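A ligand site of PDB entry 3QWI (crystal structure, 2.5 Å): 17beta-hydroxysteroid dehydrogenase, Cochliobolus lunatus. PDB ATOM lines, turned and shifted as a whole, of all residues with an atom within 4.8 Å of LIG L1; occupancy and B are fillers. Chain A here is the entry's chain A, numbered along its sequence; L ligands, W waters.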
ATOM      1  N   GLY A  25      19.198   9.232 -20.596  1.00  0.00           N
ATOM      2  CA  GLY A  25      20.549   9.503 -20.132  1.00  0.00           C
ATOM      3  C   GLY A  25      21.594   9.283 -21.215  1.00  0.00           C
ATOM      4  O   GLY A  25      22.598   8.608 -20.987  1.00  0.00           O
ATOM      5  N   SER A  26      21.350   9.833 -22.400  1.00  0.00           N
ATOM      6  CA  SER A  26      22.252   9.664 -23.535  1.00  0.00           C
ATOM      7  C   SER A  26      23.214  10.832 -23.723  1.00  0.00           C
ATOM      8  O   SER A  26      23.914  10.910 -24.737  1.00  0.00           O
ATOM      9  CB  SER A  26      21.458   9.401 -24.821  1.00  0.00           C
ATOM     10  OG  SER A  26      20.296  10.197 -24.867  1.00  0.00           O
ATOM     11  N   GLY A  27      23.270  11.725 -22.738  1.00  0.00           N
ATOM     12  CA  GLY A  27      24.225  12.819 -22.759  1.00  0.00           C
ATOM     13  C   GLY A  27      25.668  12.421 -22.513  1.00  0.00           C
ATOM     14  O   GLY A  27      26.582  13.171 -22.840  1.00  0.00           O
ATOM     15  N   ARG A  28      25.888  11.238 -21.929  1.00  0.00           N
ATOM     16  CA  ARG A  28      27.243  10.744 -21.665  1.00  0.00           C
ATOM     17  C   ARG A  28      27.263   9.228 -21.412  1.00  0.00           C
ATOM     18  O   ARG A  28      26.199   8.591 -21.364  1.00  0.00           O
ATOM     19  CB  ARG A  28      27.911  11.505 -20.499  1.00  0.00           C
ATOM     20  CG  ARG A  28      27.298  11.274 -19.125  1.00  0.00           C
ATOM     21  CD  ARG A  28      27.814  12.272 -18.062  1.00  0.00           C
ATOM     22  NE  ARG A  28      26.986  12.190 -16.853  1.00  0.00           N
ATOM     23  CZ  ARG A  28      27.292  11.515 -15.746  1.00  0.00           C
ATOM     24  NH1 ARG A  28      28.459  10.880 -15.632  1.00  0.00           N
ATOM     25  NH2 ARG A  28      26.444  11.491 -14.733  1.00  0.00           N
ATOM     26  N   GLY A  29      28.458   8.660 -21.285  1.00  0.00           N
ATOM     27  CA  GLY A  29      28.661   7.241 -20.994  1.00  0.00           C
ATOM     28  C   GLY A  29      28.114   6.318 -22.062  1.00  0.00           C
ATOM     29  O   GLY A  29      28.175   6.626 -23.261  1.00  0.00           O
ATOM     30  N   ILE A  30      27.569   5.184 -21.628  1.00  0.00           N
ATOM     31  CA  ILE A  30      26.973   4.181 -22.508  1.00  0.00           C
ATOM     32  C   ILE A  30      25.832   4.759 -23.347  1.00  0.00           C
ATOM     33  O   ILE A  30      25.771   4.527 -24.559  1.00  0.00           O
ATOM     34  CB  ILE A  30      26.458   2.951 -21.689  1.00  0.00           C
ATOM     35  CG1 ILE A  30      27.650   2.158 -21.133  1.00  0.00           C
ATOM     36  CG2 ILE A  30      25.567   2.054 -22.532  1.00  0.00           C
ATOM     37  CD1 ILE A  30      27.293   1.105 -20.090  1.00  0.00           C
ATOM     38  N   GLY A  31      24.934   5.498 -22.695  1.00  0.00           N
ATOM     39  CA  GLY A  31      23.779   6.122 -23.361  1.00  0.00           C
ATOM     40  C   GLY A  31      24.200   6.962 -24.547  1.00  0.00           C
ATOM     41  O   GLY A  31      23.562   6.891 -25.609  1.00  0.00           O
ATOM     42  N   ASN A  48      18.036  12.223 -24.269  1.00  0.00           N
ATOM     43  CA  ASN A  48      17.618  12.629 -22.930  1.00  0.00           C
ATOM     44  C   ASN A  48      18.770  12.741 -21.915  1.00  0.00           C
ATOM     45  O   ASN A  48      19.704  11.935 -21.921  1.00  0.00           O
ATOM     46  CB  ASN A  48      16.550  11.679 -22.386  1.00  0.00           C
ATOM     47  CG  ASN A  48      16.347  11.809 -20.889  1.00  0.00           C
ATOM     48  OD1 ASN A  48      16.783  10.961 -20.127  1.00  0.00           O
ATOM     49  ND2 ASN A  48      15.707  12.896 -20.469  1.00  0.00           N
ATOM     50  N   TYR A  49      18.666  13.751 -21.059  1.00  0.00           N
ATOM     51  CA  TYR A  49      19.617  14.008 -20.000  1.00  0.00           C
ATOM     52  C   TYR A  49      18.853  14.591 -18.829  1.00  0.00           C
ATOM     53  O   TYR A  49      17.743  15.093 -19.002  1.00  0.00           O
ATOM     54  CB  TYR A  49      20.661  15.015 -20.469  1.00  0.00           C
ATOM     55  CG  TYR A  49      20.133  16.412 -20.779  1.00  0.00           C
ATOM     56  CD1 TYR A  49      19.520  16.694 -22.004  1.00  0.00           C
ATOM     57  CD2 TYR A  49      20.268  17.460 -19.859  1.00  0.00           C
ATOM     58  CE1 TYR A  49      19.041  17.974 -22.292  1.00  0.00           C
ATOM     59  CE2 TYR A  49      19.790  18.740 -20.137  1.00  0.00           C
ATOM     60  CZ  TYR A  49      19.188  18.988 -21.365  1.00  0.00           C
ATOM     61  OH  TYR A  49      18.720  20.247 -21.654  1.00  0.00           O
ATOM     62  N   ALA A  50      19.439  14.535 -17.632  1.00  0.00           N
ATOM     63  CA  ALA A  50      18.882  15.235 -16.483  1.00  0.00           C
ATOM     64  C   ALA A  50      19.696  16.483 -16.110  1.00  0.00           C
ATOM     65  O   ALA A  50      19.132  17.484 -15.647  1.00  0.00           O
ATOM     66  CB  ALA A  50      18.793  14.298 -15.305  1.00  0.00           C
ATOM     67  N   ASN A  51      21.015  16.411 -16.324  1.00  0.00           N
ATOM     68  CA  ASN A  51      21.968  17.419 -15.838  1.00  0.00           C
ATOM     69  C   ASN A  51      23.012  17.838 -16.868  1.00  0.00           C
ATOM     70  O   ASN A  51      23.440  18.992 -16.886  1.00  0.00           O
ATOM     71  CB  ASN A  51      22.678  16.919 -14.587  1.00  0.00           C
ATOM     72  CG  ASN A  51      21.719  16.597 -13.455  1.00  0.00           C
ATOM     73  OD1 ASN A  51      21.194  17.499 -12.788  1.00  0.00           O
ATOM     74  ND2 ASN A  51      21.478  15.302 -13.221  1.00  0.00           N
ATOM     75  N   SER A  52      23.406  16.904 -17.732  1.00  0.00           N
ATOM     76  CA  SER A  52      24.482  17.129 -18.693  1.00  0.00           C
ATOM     77  C   SER A  52      24.035  17.792 -20.005  1.00  0.00           C
ATOM     78  O   SER A  52      24.004  17.161 -21.048  1.00  0.00           O
ATOM     79  CB  SER A  52      25.203  15.808 -18.967  1.00  0.00           C
ATOM     80  OG  SER A  52      25.623  15.220 -17.760  1.00  0.00           O
ATOM     81  N   ALA A  75      14.781  15.800 -19.075  1.00  0.00           N
ATOM     82  CA  ALA A  75      13.770  15.180 -18.197  1.00  0.00           C
ATOM     83  C   ALA A  75      14.440  14.306 -17.124  1.00  0.00           C
ATOM     84  O   ALA A  75      15.334  13.512 -17.418  1.00  0.00           O
ATOM     85  CB  ALA A  75      12.756  14.366 -18.991  1.00  0.00           C
ATOM     86  N   ASP A  76      13.990  14.472 -15.886  1.00  0.00           N
ATOM     87  CA  ASP A  76      14.465  13.701 -14.741  1.00  0.00           C
ATOM     88  C   ASP A  76      13.687  12.388 -14.657  1.00  0.00           C
ATOM     89  O   ASP A  76      12.512  12.369 -14.273  1.00  0.00           O
ATOM     90  CB  ASP A  76      14.297  14.523 -13.450  1.00  0.00           C
ATOM     91  CG  ASP A  76      14.634  13.743 -12.180  1.00  0.00           C
ATOM     92  OD1 ASP A  76      15.102  12.581 -12.236  1.00  0.00           O
ATOM     93  OD2 ASP A  76      14.437  14.325 -11.101  1.00  0.00           O
ATOM     94  N   ILE A  77      14.359  11.287 -14.999  1.00  0.00           N
ATOM     95  CA  ILE A  77      13.685   9.999 -15.149  1.00  0.00           C
ATOM     96  C   ILE A  77      13.132   9.415 -13.835  1.00  0.00           C
ATOM     97  O   ILE A  77      12.337   8.463 -13.863  1.00  0.00           O
ATOM     98  CB  ILE A  77      14.566   8.984 -15.985  1.00  0.00           C
ATOM     99  CG1 ILE A  77      14.768   9.492 -17.420  1.00  0.00           C
ATOM    100  CG2 ILE A  77      13.927   7.603 -16.051  1.00  0.00           C
ATOM    101  CD1 ILE A  77      13.479   9.626 -18.256  1.00  0.00           C
ATOM    102  N   ARG A  78      13.520  10.002 -12.698  1.00  0.00           N
ATOM    103  CA  ARG A  78      12.911   9.655 -11.410  1.00  0.00           C
ATOM    104  C   ARG A  78      11.461  10.090 -11.303  1.00  0.00           C
ATOM    105  O   ARG A  78      10.684   9.503 -10.542  1.00  0.00           O
ATOM    106  CB  ARG A  78      13.714  10.232 -10.249  1.00  0.00           C
ATOM    107  CG  ARG A  78      14.951   9.421  -9.915  1.00  0.00           C
ATOM    108  CD  ARG A  78      15.592   9.895  -8.633  1.00  0.00           C
ATOM    109  NE  ARG A  78      16.796   9.111  -8.347  1.00  0.00           N
ATOM    110  CZ  ARG A  78      18.039   9.497  -8.625  1.00  0.00           C
ATOM    111  NH1 ARG A  78      18.268  10.680  -9.195  1.00  0.00           N
ATOM    112  NH2 ARG A  78      19.059   8.706  -8.333  1.00  0.00           N
ATOM    113  N   ASN A 103      18.347   3.618 -20.347  1.00  0.00           N
ATOM    114  CA  ASN A 103      19.767   3.493 -20.046  1.00  0.00           C
ATOM    115  C   ASN A 103      20.178   4.174 -18.745  1.00  0.00           C
ATOM    116  O   ASN A 103      21.056   3.680 -18.041  1.00  0.00           O
ATOM    117  CB  ASN A 103      20.609   4.024 -21.214  1.00  0.00           C
ATOM    118  CG  ASN A 103      22.005   4.438 -20.794  1.00  0.00           C
ATOM    119  OD1 ASN A 103      22.890   3.604 -20.640  1.00  0.00           O
ATOM    120  ND2 ASN A 103      22.195   5.740 -20.605  1.00  0.00           N
ATOM    121  N   SER A 104      19.560   5.298 -18.424  1.00  0.00           N
ATOM    122  CA  SER A 104      19.835   6.024 -17.185  1.00  0.00           C
ATOM    123  C   SER A 104      19.887   5.115 -15.971  1.00  0.00           C
ATOM    124  O   SER A 104      19.010   4.250 -15.801  1.00  0.00           O
ATOM    125  CB  SER A 104      18.778   7.102 -16.951  1.00  0.00           C
ATOM    126  OG  SER A 104      19.031   8.183 -17.817  1.00  0.00           O
ATOM    127  N   GLY A 105      20.909   5.308 -15.148  1.00  0.00           N
ATOM    128  CA  GLY A 105      21.102   4.529 -13.932  1.00  0.00           C
ATOM    129  C   GLY A 105      22.172   5.130 -13.050  1.00  0.00           C
ATOM    130  O   GLY A 105      22.980   5.953 -13.510  1.00  0.00           O
ATOM    131  N   VAL A 106      22.158   4.744 -11.767  1.00  0.00           N
ATOM    132  CA  VAL A 106      23.208   5.104 -10.816  1.00  0.00           C
ATOM    133  C   VAL A 106      23.688   3.864 -10.076  1.00  0.00           C
ATOM    134  O   VAL A 106      22.930   2.892  -9.916  1.00  0.00           O
ATOM    135  CB  VAL A 106      22.780   6.188  -9.773  1.00  0.00           C
ATOM    136  CG1 VAL A 106      22.572   7.555 -10.428  1.00  0.00           C
ATOM    137  CG2 VAL A 106      21.541   5.739  -8.968  1.00  0.00           C
ATOM    138  N   LEU A 126      15.412   5.449  -9.683  1.00  0.00           N
ATOM    139  CA  LEU A 126      15.953   5.571 -11.050  1.00  0.00           C
ATOM    140  C   LEU A 126      16.100   4.230 -11.765  1.00  0.00           C
ATOM    141  O   LEU A 126      15.524   4.045 -12.834  1.00  0.00           O
ATOM    142  CB  LEU A 126      17.291   6.309 -11.063  1.00  0.00           C
ATOM    143  CG  LEU A 126      17.863   6.650 -12.450  1.00  0.00           C
ATOM    144  CD1 LEU A 126      16.932   7.585 -13.229  1.00  0.00           C
ATOM    145  CD2 LEU A 126      19.251   7.231 -12.343  1.00  0.00           C
ATOM    146  N   THR A 151      18.151  -1.639 -19.253  1.00  0.00           N
ATOM    147  CA  THR A 151      19.535  -1.864 -18.886  1.00  0.00           C
ATOM    148  C   THR A 151      19.677  -2.592 -17.545  1.00  0.00           C
ATOM    149  O   THR A 151      19.213  -2.118 -16.502  1.00  0.00           O
ATOM    150  CB  THR A 151      20.323  -0.549 -18.869  1.00  0.00           C
ATOM    151  OG1 THR A 151      20.156   0.120 -20.122  1.00  0.00           O
ATOM    152  CG2 THR A 151      21.793  -0.815 -18.637  1.00  0.00           C
ATOM    153  N   SER A 152      20.330  -3.749 -17.578  1.00  0.00           N
ATOM    154  CA  SER A 152      20.590  -4.492 -16.353  1.00  0.00           C
ATOM    155  C   SER A 152      22.088  -4.411 -16.005  1.00  0.00           C
ATOM    156  O   SER A 152      22.716  -3.361 -16.166  1.00  0.00           O
ATOM    157  CB  SER A 152      20.120  -5.942 -16.499  1.00  0.00           C
ATOM    158  OG  SER A 152      20.174  -6.623 -15.263  1.00  0.00           O
ATOM    159  N   SER A 153      22.638  -5.522 -15.531  1.00  0.00           N
ATOM    160  CA  SER A 153      23.991  -5.560 -15.003  1.00  0.00           C
ATOM    161  C   SER A 153      24.458  -7.005 -14.983  1.00  0.00           C
ATOM    162  O   SER A 153      23.643  -7.907 -14.778  1.00  0.00           O
ATOM    163  CB  SER A 153      23.967  -5.021 -13.572  1.00  0.00           C
ATOM    164  OG  SER A 153      25.212  -4.434 -13.238  1.00  0.00           O
ATOM    165  N   TYR A 167      22.315  -2.381  -5.510  1.00  0.00           N
ATOM    166  CA  TYR A 167      22.410  -2.184  -6.957  1.00  0.00           C
ATOM    167  C   TYR A 167      22.078  -3.463  -7.720  1.00  0.00           C
ATOM    168  O   TYR A 167      21.352  -3.428  -8.703  1.00  0.00           O
ATOM    169  CB  TYR A 167      23.806  -1.676  -7.334  1.00  0.00           C
ATOM    170  CG  TYR A 167      24.023  -1.499  -8.816  1.00  0.00           C
ATOM    171  CD1 TYR A 167      23.597  -0.342  -9.473  1.00  0.00           C
ATOM    172  CD2 TYR A 167      24.683  -2.480  -9.562  1.00  0.00           C
ATOM    173  CE1 TYR A 167      23.818  -0.170 -10.846  1.00  0.00           C
ATOM    174  CE2 TYR A 167      24.898  -2.316 -10.925  1.00  0.00           C
ATOM    175  CZ  TYR A 167      24.467  -1.169 -11.562  1.00  0.00           C
ATOM    176  OH  TYR A 167      24.692  -1.026 -12.906  1.00  0.00           O
ATOM    177  N   LYS A 171      18.747  -4.183 -10.487  1.00  0.00           N
ATOM    178  CA  LYS A 171      18.821  -4.699 -11.848  1.00  0.00           C
ATOM    179  C   LYS A 171      18.164  -6.078 -11.993  1.00  0.00           C
ATOM    180  O   LYS A 171      17.731  -6.452 -13.088  1.00  0.00           O
ATOM    181  CB  LYS A 171      20.272  -4.692 -12.333  1.00  0.00           C
ATOM    182  CG  LYS A 171      20.905  -3.291 -12.387  1.00  0.00           C
ATOM    183  CD  LYS A 171      20.001  -2.264 -13.102  1.00  0.00           C
ATOM    184  CE  LYS A 171      20.694  -0.921 -13.281  1.00  0.00           C
ATOM    185  NZ  LYS A 171      21.646  -0.912 -14.438  1.00  0.00           N
ATOM    186  N   PRO A 197      25.510  -5.072 -19.183  1.00  0.00           N
ATOM    187  CA  PRO A 197      26.960  -4.905 -19.330  1.00  0.00           C
ATOM    188  C   PRO A 197      27.744  -5.361 -18.090  1.00  0.00           C
ATOM    189  O   PRO A 197      27.224  -5.367 -16.979  1.00  0.00           O
ATOM    190  CB  PRO A 197      27.121  -3.394 -19.520  1.00  0.00           C
ATOM    191  CG  PRO A 197      25.738  -2.863 -19.852  1.00  0.00           C
ATOM    192  CD  PRO A 197      24.792  -3.786 -19.171  1.00  0.00           C
ATOM    193  N   GLY A 198      29.000  -5.754 -18.318  1.00  0.00           N
ATOM    194  CA  GLY A 198      29.975  -5.886 -17.249  1.00  0.00           C
ATOM    195  C   GLY A 198      30.709  -4.569 -17.130  1.00  0.00           C
ATOM    196  O   GLY A 198      30.211  -3.525 -17.569  1.00  0.00           O
ATOM    197  N   GLY A 199      31.901  -4.608 -16.535  1.00  0.00           N
ATOM    198  CA  GLY A 199      32.720  -3.409 -16.416  1.00  0.00           C
ATOM    199  C   GLY A 199      32.960  -2.717 -17.742  1.00  0.00           C
ATOM    200  O   GLY A 199      33.732  -3.210 -18.578  1.00  0.00           O
ATOM    201  N   THR A 200      32.309  -1.570 -17.930  1.00  0.00           N
ATOM    202  CA  THR A 200      32.392  -0.781 -19.146  1.00  0.00           C
ATOM    203  C   THR A 200      32.978   0.586 -18.798  1.00  0.00           C
ATOM    204  O   THR A 200      32.525   1.246 -17.866  1.00  0.00           O
ATOM    205  CB  THR A 200      30.986  -0.621 -19.776  1.00  0.00           C
ATOM    206  OG1 THR A 200      30.341  -1.896 -19.836  1.00  0.00           O
ATOM    207  CG2 THR A 200      31.060  -0.051 -21.183  1.00  0.00           C
ATOM    208  N   THR A 202      33.448   4.087 -18.358  1.00  0.00           N
ATOM    209  CA  THR A 202      32.699   5.332 -18.317  1.00  0.00           C
ATOM    210  C   THR A 202      32.969   5.958 -16.953  1.00  0.00           C
ATOM    211  O   THR A 202      33.722   5.394 -16.158  1.00  0.00           O
ATOM    212  CB  THR A 202      31.154   5.118 -18.410  1.00  0.00           C
ATOM    213  OG1 THR A 202      30.711   4.411 -17.247  1.00  0.00           O
ATOM    214  CG2 THR A 202      30.747   4.356 -19.666  1.00  0.00           C
ATOM    215  N   ASP A 203      32.342   7.089 -16.662  1.00  0.00           N
ATOM    216  CA  ASP A 203      32.398   7.706 -15.330  1.00  0.00           C
ATOM    217  C   ASP A 203      31.976   6.741 -14.201  1.00  0.00           C
ATOM    218  O   ASP A 203      32.548   6.775 -13.108  1.00  0.00           O
ATOM    219  CB  ASP A 203      31.560   8.985 -15.304  1.00  0.00           C
ATOM    220  CG  ASP A 203      32.094  10.074 -16.251  1.00  0.00           C
ATOM    221  OD1 ASP A 203      33.339  10.162 -16.423  1.00  0.00           O
ATOM    222  OD2 ASP A 203      31.276  10.838 -16.802  1.00  0.00           O
ATOM    223  N   MET A 204      30.984   5.887 -14.467  1.00  0.00           N
ATOM    224  CA  MET A 204      30.560   4.900 -13.479  1.00  0.00           C
ATOM    225  C   MET A 204      31.680   3.940 -13.129  1.00  0.00           C
ATOM    226  O   MET A 204      31.846   3.567 -11.961  1.00  0.00           O
ATOM    227  CB  MET A 204      29.340   4.117 -13.953  1.00  0.00           C
ATOM    228  CG  MET A 204      28.817   3.144 -12.911  1.00  0.00           C
ATOM    229  SD  MET A 204      27.200   2.482 -13.294  1.00  0.00           S
ATOM    230  CE  MET A 204      26.167   3.922 -12.992  1.00  0.00           C
ATOM    231  N   PHE A 205      32.422   3.524 -14.150  1.00  0.00           N
ATOM    232  CA  PHE A 205      33.545   2.616 -13.967  1.00  0.00           C
ATOM    233  C   PHE A 205      34.534   3.202 -12.963  1.00  0.00           C
ATOM    234  O   PHE A 205      34.876   2.553 -11.987  1.00  0.00           O
ATOM    235  CB  PHE A 205      34.210   2.282 -15.312  1.00  0.00           C
ATOM    236  CG  PHE A 205      35.240   1.168 -15.217  1.00  0.00           C
ATOM    237  CD1 PHE A 205      36.563   1.451 -14.892  1.00  0.00           C
ATOM    238  CD2 PHE A 205      34.873  -0.158 -15.461  1.00  0.00           C
ATOM    239  CE1 PHE A 205      37.511   0.428 -14.799  1.00  0.00           C
ATOM    240  CE2 PHE A 205      35.814  -1.188 -15.378  1.00  0.00           C
ATOM    241  CZ  PHE A 205      37.136  -0.892 -15.042  1.00  0.00           C
HETATM  242  P1  LIG L   1      27.406   6.976 -16.170  1.00  0.00           P
HETATM  243  O1  LIG L   1      27.548   7.370 -14.753  1.00  0.00           O
HETATM  244  O2  LIG L   1      28.563   7.136 -17.078  1.00  0.00           O
HETATM  245  O3  LIG L   1      26.154   7.716 -16.807  1.00  0.00           O
HETATM  246  C1  LIG L   1      24.881   7.691 -16.159  1.00  0.00           C
HETATM  247  C2  LIG L   1      23.791   8.231 -17.093  1.00  0.00           C
HETATM  248  O4  LIG L   1      22.509   8.188 -16.385  1.00  0.00           O
HETATM  249  C3  LIG L   1      24.050   9.706 -17.459  1.00  0.00           C
HETATM  250  O5  LIG L   1      23.710   9.928 -18.837  1.00  0.00           O
HETATM  251  C4  LIG L   1      23.087  10.465 -16.542  1.00  0.00           C
HETATM  252  O6  LIG L   1      22.662  11.696 -17.125  1.00  0.00           O
HETATM  253  C5  LIG L   1      21.896   9.508 -16.506  1.00  0.00           C
HETATM  254  N1  LIG L   1      21.046   9.903 -15.351  1.00  0.00           N
HETATM  255  C6  LIG L   1      21.406   9.923 -14.051  1.00  0.00           C
HETATM  256  N2  LIG L   1      20.375  10.356 -13.319  1.00  0.00           N
HETATM  257  C7  LIG L   1      19.358  10.607 -14.150  1.00  0.00           C
HETATM  258  C8  LIG L   1      18.065  11.055 -13.978  1.00  0.00           C
HETATM  259  N3  LIG L   1      17.600  11.349 -12.764  1.00  0.00           N
HETATM  260  N4  LIG L   1      17.272  11.209 -15.063  1.00  0.00           N
HETATM  261  C9  LIG L   1      17.720  10.943 -16.286  1.00  0.00           C
HETATM  262  N5  LIG L   1      18.960  10.511 -16.484  1.00  0.00           N
HETATM  263  C10 LIG L   1      19.791  10.328 -15.443  1.00  0.00           C
HETATM  264  O7  LIG L   1      26.924   5.430 -16.160  1.00  0.00           O
HETATM  265  P2  LIG L   1      26.987   4.461 -17.464  1.00  0.00           P
HETATM  266  O8  LIG L   1      26.653   5.225 -18.706  1.00  0.00           O
HETATM  267  O9  LIG L   1      28.247   3.689 -17.391  1.00  0.00           O
HETATM  268  O10 LIG L   1      25.755   3.505 -17.146  1.00  0.00           O
HETATM  269  C11 LIG L   1      24.568   3.519 -17.922  1.00  0.00           C
HETATM  270  C12 LIG L   1      23.726   2.289 -17.531  1.00  0.00           C
HETATM  271  O11 LIG L   1      24.549   1.114 -17.652  1.00  0.00           O
HETATM  272  C13 LIG L   1      23.286   2.366 -16.078  1.00  0.00           C
HETATM  273  O12 LIG L   1      21.966   1.854 -16.004  1.00  0.00           O
HETATM  274  C14 LIG L   1      24.252   1.418 -15.381  1.00  0.00           C
HETATM  275  O13 LIG L   1      23.685   0.861 -14.195  1.00  0.00           O
HETATM  276  C15 LIG L   1      24.420   0.348 -16.443  1.00  0.00           C
HETATM  277  N6  LIG L   1      25.682  -0.402 -16.238  1.00  0.00           N
HETATM  278  C16 LIG L   1      26.945   0.218 -16.345  1.00  0.00           C
HETATM  279  C17 LIG L   1      28.101  -0.538 -16.136  1.00  0.00           C
HETATM  280  C18 LIG L   1      29.509   0.057 -16.259  1.00  0.00           C
HETATM  281  O14 LIG L   1      30.598  -0.747 -16.091  1.00  0.00           O
HETATM  282  N7  LIG L   1      29.628   1.349 -16.559  1.00  0.00           N
HETATM  283  C19 LIG L   1      27.998  -1.893 -15.820  1.00  0.00           C
HETATM  284  C20 LIG L   1      26.755  -2.505 -15.704  1.00  0.00           C
HETATM  285  C21 LIG L   1      25.595  -1.770 -15.913  1.00  0.00           C
HETATM  286  P3  LIG L   1      22.958  13.133 -16.453  1.00  0.00           P
HETATM  287  O15 LIG L   1      22.400  14.219 -17.278  1.00  0.00           O
HETATM  288  O16 LIG L   1      24.537  13.255 -16.296  1.00  0.00           O
HETATM  289  O17 LIG L   1      22.380  13.127 -14.958  1.00  0.00           O
HETATM  290  O1  LG2 L   2      32.407  -6.641 -13.631  1.00  0.00           O
HETATM  291  O2  LG2 L   2      29.340  -0.412 -12.990  1.00  0.00           O
HETATM  292  O3  LG2 L   2      38.967  -6.409 -11.863  1.00  0.00           O
HETATM  293  C1  LG2 L   2      31.717  -0.596 -12.618  1.00  0.00           C
HETATM  294  C2  LG2 L   2      36.798  -7.164 -12.501  1.00  0.00           C
HETATM  295  C3  LG2 L   2      32.858  -1.389 -12.541  1.00  0.00           C
HETATM  296  C4  LG2 L   2      35.458  -6.860 -12.776  1.00  0.00           C
HETATM  297  C5  LG2 L   2      30.388  -2.544 -13.138  1.00  0.00           C
HETATM  298  C6  LG2 L   2      37.210  -4.818 -12.047  1.00  0.00           C
HETATM  299  O4  LG2 L   2      31.381  -4.696 -13.284  1.00  0.00           O
HETATM  300  O5  LG2 L   2      35.192  -3.337 -12.317  1.00  0.00           O
HETATM  301  C7  LG2 L   2      30.485  -1.170 -12.911  1.00  0.00           C
HETATM  302  C8  LG2 L   2      37.666  -6.136 -12.141  1.00  0.00           C
HETATM  303  C9  LG2 L   2      32.510  -5.466 -13.275  1.00  0.00           C
HETATM  304  C10 LG2 L   2      31.523  -3.345 -13.061  1.00  0.00           C
HETATM  305  C11 LG2 L   2      35.877  -4.520 -12.332  1.00  0.00           C
HETATM  306  C12 LG2 L   2      32.768  -2.769 -12.788  1.00  0.00           C
HETATM  307  C13 LG2 L   2      35.002  -5.541 -12.692  1.00  0.00           C
HETATM  308  C14 LG2 L   2      33.892  -3.587 -12.681  1.00  0.00           C
HETATM  309  C15 LG2 L   2      33.751  -4.952 -12.905  1.00  0.00           C
HETATM  310  O   HOH W   1      24.927   6.486 -20.210  1.00  0.00           O
HETATM  311  O   HOH W   2      16.757  13.162 -10.035  1.00  0.00           O
HETATM  312  O   HOH W   3      27.645  -4.377 -13.117  1.00  0.00           O
HETATM  313  O   HOH W   4      28.792   8.606 -13.004  1.00  0.00           O
HETATM  314  O   HOH W   5      22.819  12.495 -19.786  1.00  0.00           O
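The backbone NH (N) of Asn 51 is in hydrogen-bond range of an oxygen (O15) of LIG L1 (2.8 Å). An oxygen (O8) of LIG L1 sits at hydrogen-bond distance from the backbone NH of Ile 30, at 3.1 Å. O15 of LIG L1 sits at hydrogen-bond distance from N of Ala 50 (3.0 Å). The side-chain hydroxyl of Ser 104 is in hydrogen-bond range of a nitrogen (N5) of LIG L1, at 2.7 Å. The backbone carbonyl oxygen (O) of Thr 200 sits at hydrogen-bond distance from a nitrogen (N7) of LIG L1 (3.2 Å). N of Gly 199 lies within hydrogen-bond range of O4 of LG2 L2 (3.3 Å). The side-chain hydroxyl (OH) of Tyr 167 sits at hydrogen-bond distance from an oxygen (O13) of LIG L1, at 2.5 Å. NE of Arg 28 lies within salt-bridge range of O16 of LIG L1 (2.7 Å). An oxygen (O14) of LIG L1 is in hydrogen-bond range of the backbone NH of Thr 200 (2.6 Å). O12 of LIG L1 is in hydrogen-bond range of O of Asn 103 (2.9 Å). The side-chain amino group of Lys 171 is in hydrogen-bond range of an oxygen (O13) of LIG L1, at 2.7 Å. O2 of LG2 L2 sits close to SD of Met 204, at 3.6 Å. OG1 of Thr 202 sits at hydrogen-bond distance from O9 of LIG L1 (2.6 Å). The backbone NH of Ser 52 lies within hydrogen-bond range of an oxygen (O15) of LIG L1. The backbone carbonyl oxygen (O) of Gly 25 lies within hydrogen-bond range of an oxygen (O5) of LIG L1 (2.8 Å). A nitrogen (N4) of LIG L1 is in hydrogen-bond range of the backbone NH (N) of Ile 77 (2.9 Å). ND2 of Asn 51 lies within hydrogen-bond range of O17 of LIG L1 (2.9 Å). OG of Ser 52 lies within hydrogen-bond range of O16 of LIG L1 (2.7 Å). The side-chain carboxylate (OD1) of Asp 76 is in hydrogen-bond range of a nitrogen (N3) of LIG L1 (2.8 Å).
An oxygen (O2) of LG2 L2 lies close to an oxygen (O14) of LIG L1 (3.4 Å).
The side-chain amide nitrogen (ND2) of Asn 103 sits close to the backbone NH (N) of Gly 31 (3.5 Å). The backbone carbonyl oxygen (O) of Asn 48 lies within hydrogen-bond range of the backbone NH (N) of Ser 26 (2.7 Å). The side-chain hydroxyl of Tyr 167 is in hydrogen-bond range of the side-chain amino group of Lys 171 (3.4 Å). ND2 of Asn 103 lies within hydrogen-bond range of O of Gly 25. The side-chain hydroxyl of Thr 200 sits at hydrogen-bond distance from the backbone carbonyl oxygen of Gly 198 (2.8 Å). NZ of Lys 171 lies within hydrogen-bond range of O of Thr 151, at 3.4 Å. N of Ala 75 sits at hydrogen-bond distance from O of Tyr 49 (3.0 Å). The backbone NH (N) of Met 204 lies within hydrogen-bond range of the side-chain hydroxyl (OG1) of Thr 202 (3.2 Å).
O14 of LIG L1 lies close to O of Gly 198 (3.2 Å). CA of Gly 29 touches O8 of LIG L1, at 3.7 Å. Asn 48 touches LIG L1. Tyr 49 touches LIG L1 (CB to O15, 3.7 Å). Ala 75 touches LIG L1 (O to C9, 3.7 Å). Arg 78 touches LIG L1 (NH1 to N3, 3.7 Å). Gly 105 touches LIG L1. CD2 of Leu 126 touches N2 of LIG L1, 3.5 Å away. CG2 of Thr 151 touches O11 of LIG L1 (3.5 Å). O of Ser 152 touches C21 of LIG L1, 3.3 Å away. OG of Ser 153 touches C20 of LIG L1 (3.5 Å). Pro 197 touches LIG L1. CA of Gly 199 touches O14 of LIG L1 (3.4 Å). Asp 203 touches LIG L1 (N to O2, 3.8 Å). CB of Met 204 touches O7 of LIG L1, 3.5 Å away. The nearest printed residue that does not touch LIG L1 is Ser 26 (4.3 Å).
Water W4 lies within hydrogen-bond range of an oxygen (O1) of LIG L1 (2.5 Å) and the guanidinium group (NH1) of Arg 28 (3.5 Å). Water W5 bridges an oxygen (O6) of LIG L1 (2.8 Å) and the backbone NH (N) of Gly 27 (3.1 Å). Water W2 lies within hydrogen-bond range of the side-chain carboxylate (OD2) of Asp 76 (2.8 Å), the guanidinium group (NH1) of Arg 78 (3.0 Å) and a nitrogen (N3) of LIG L1 (3.4 Å).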
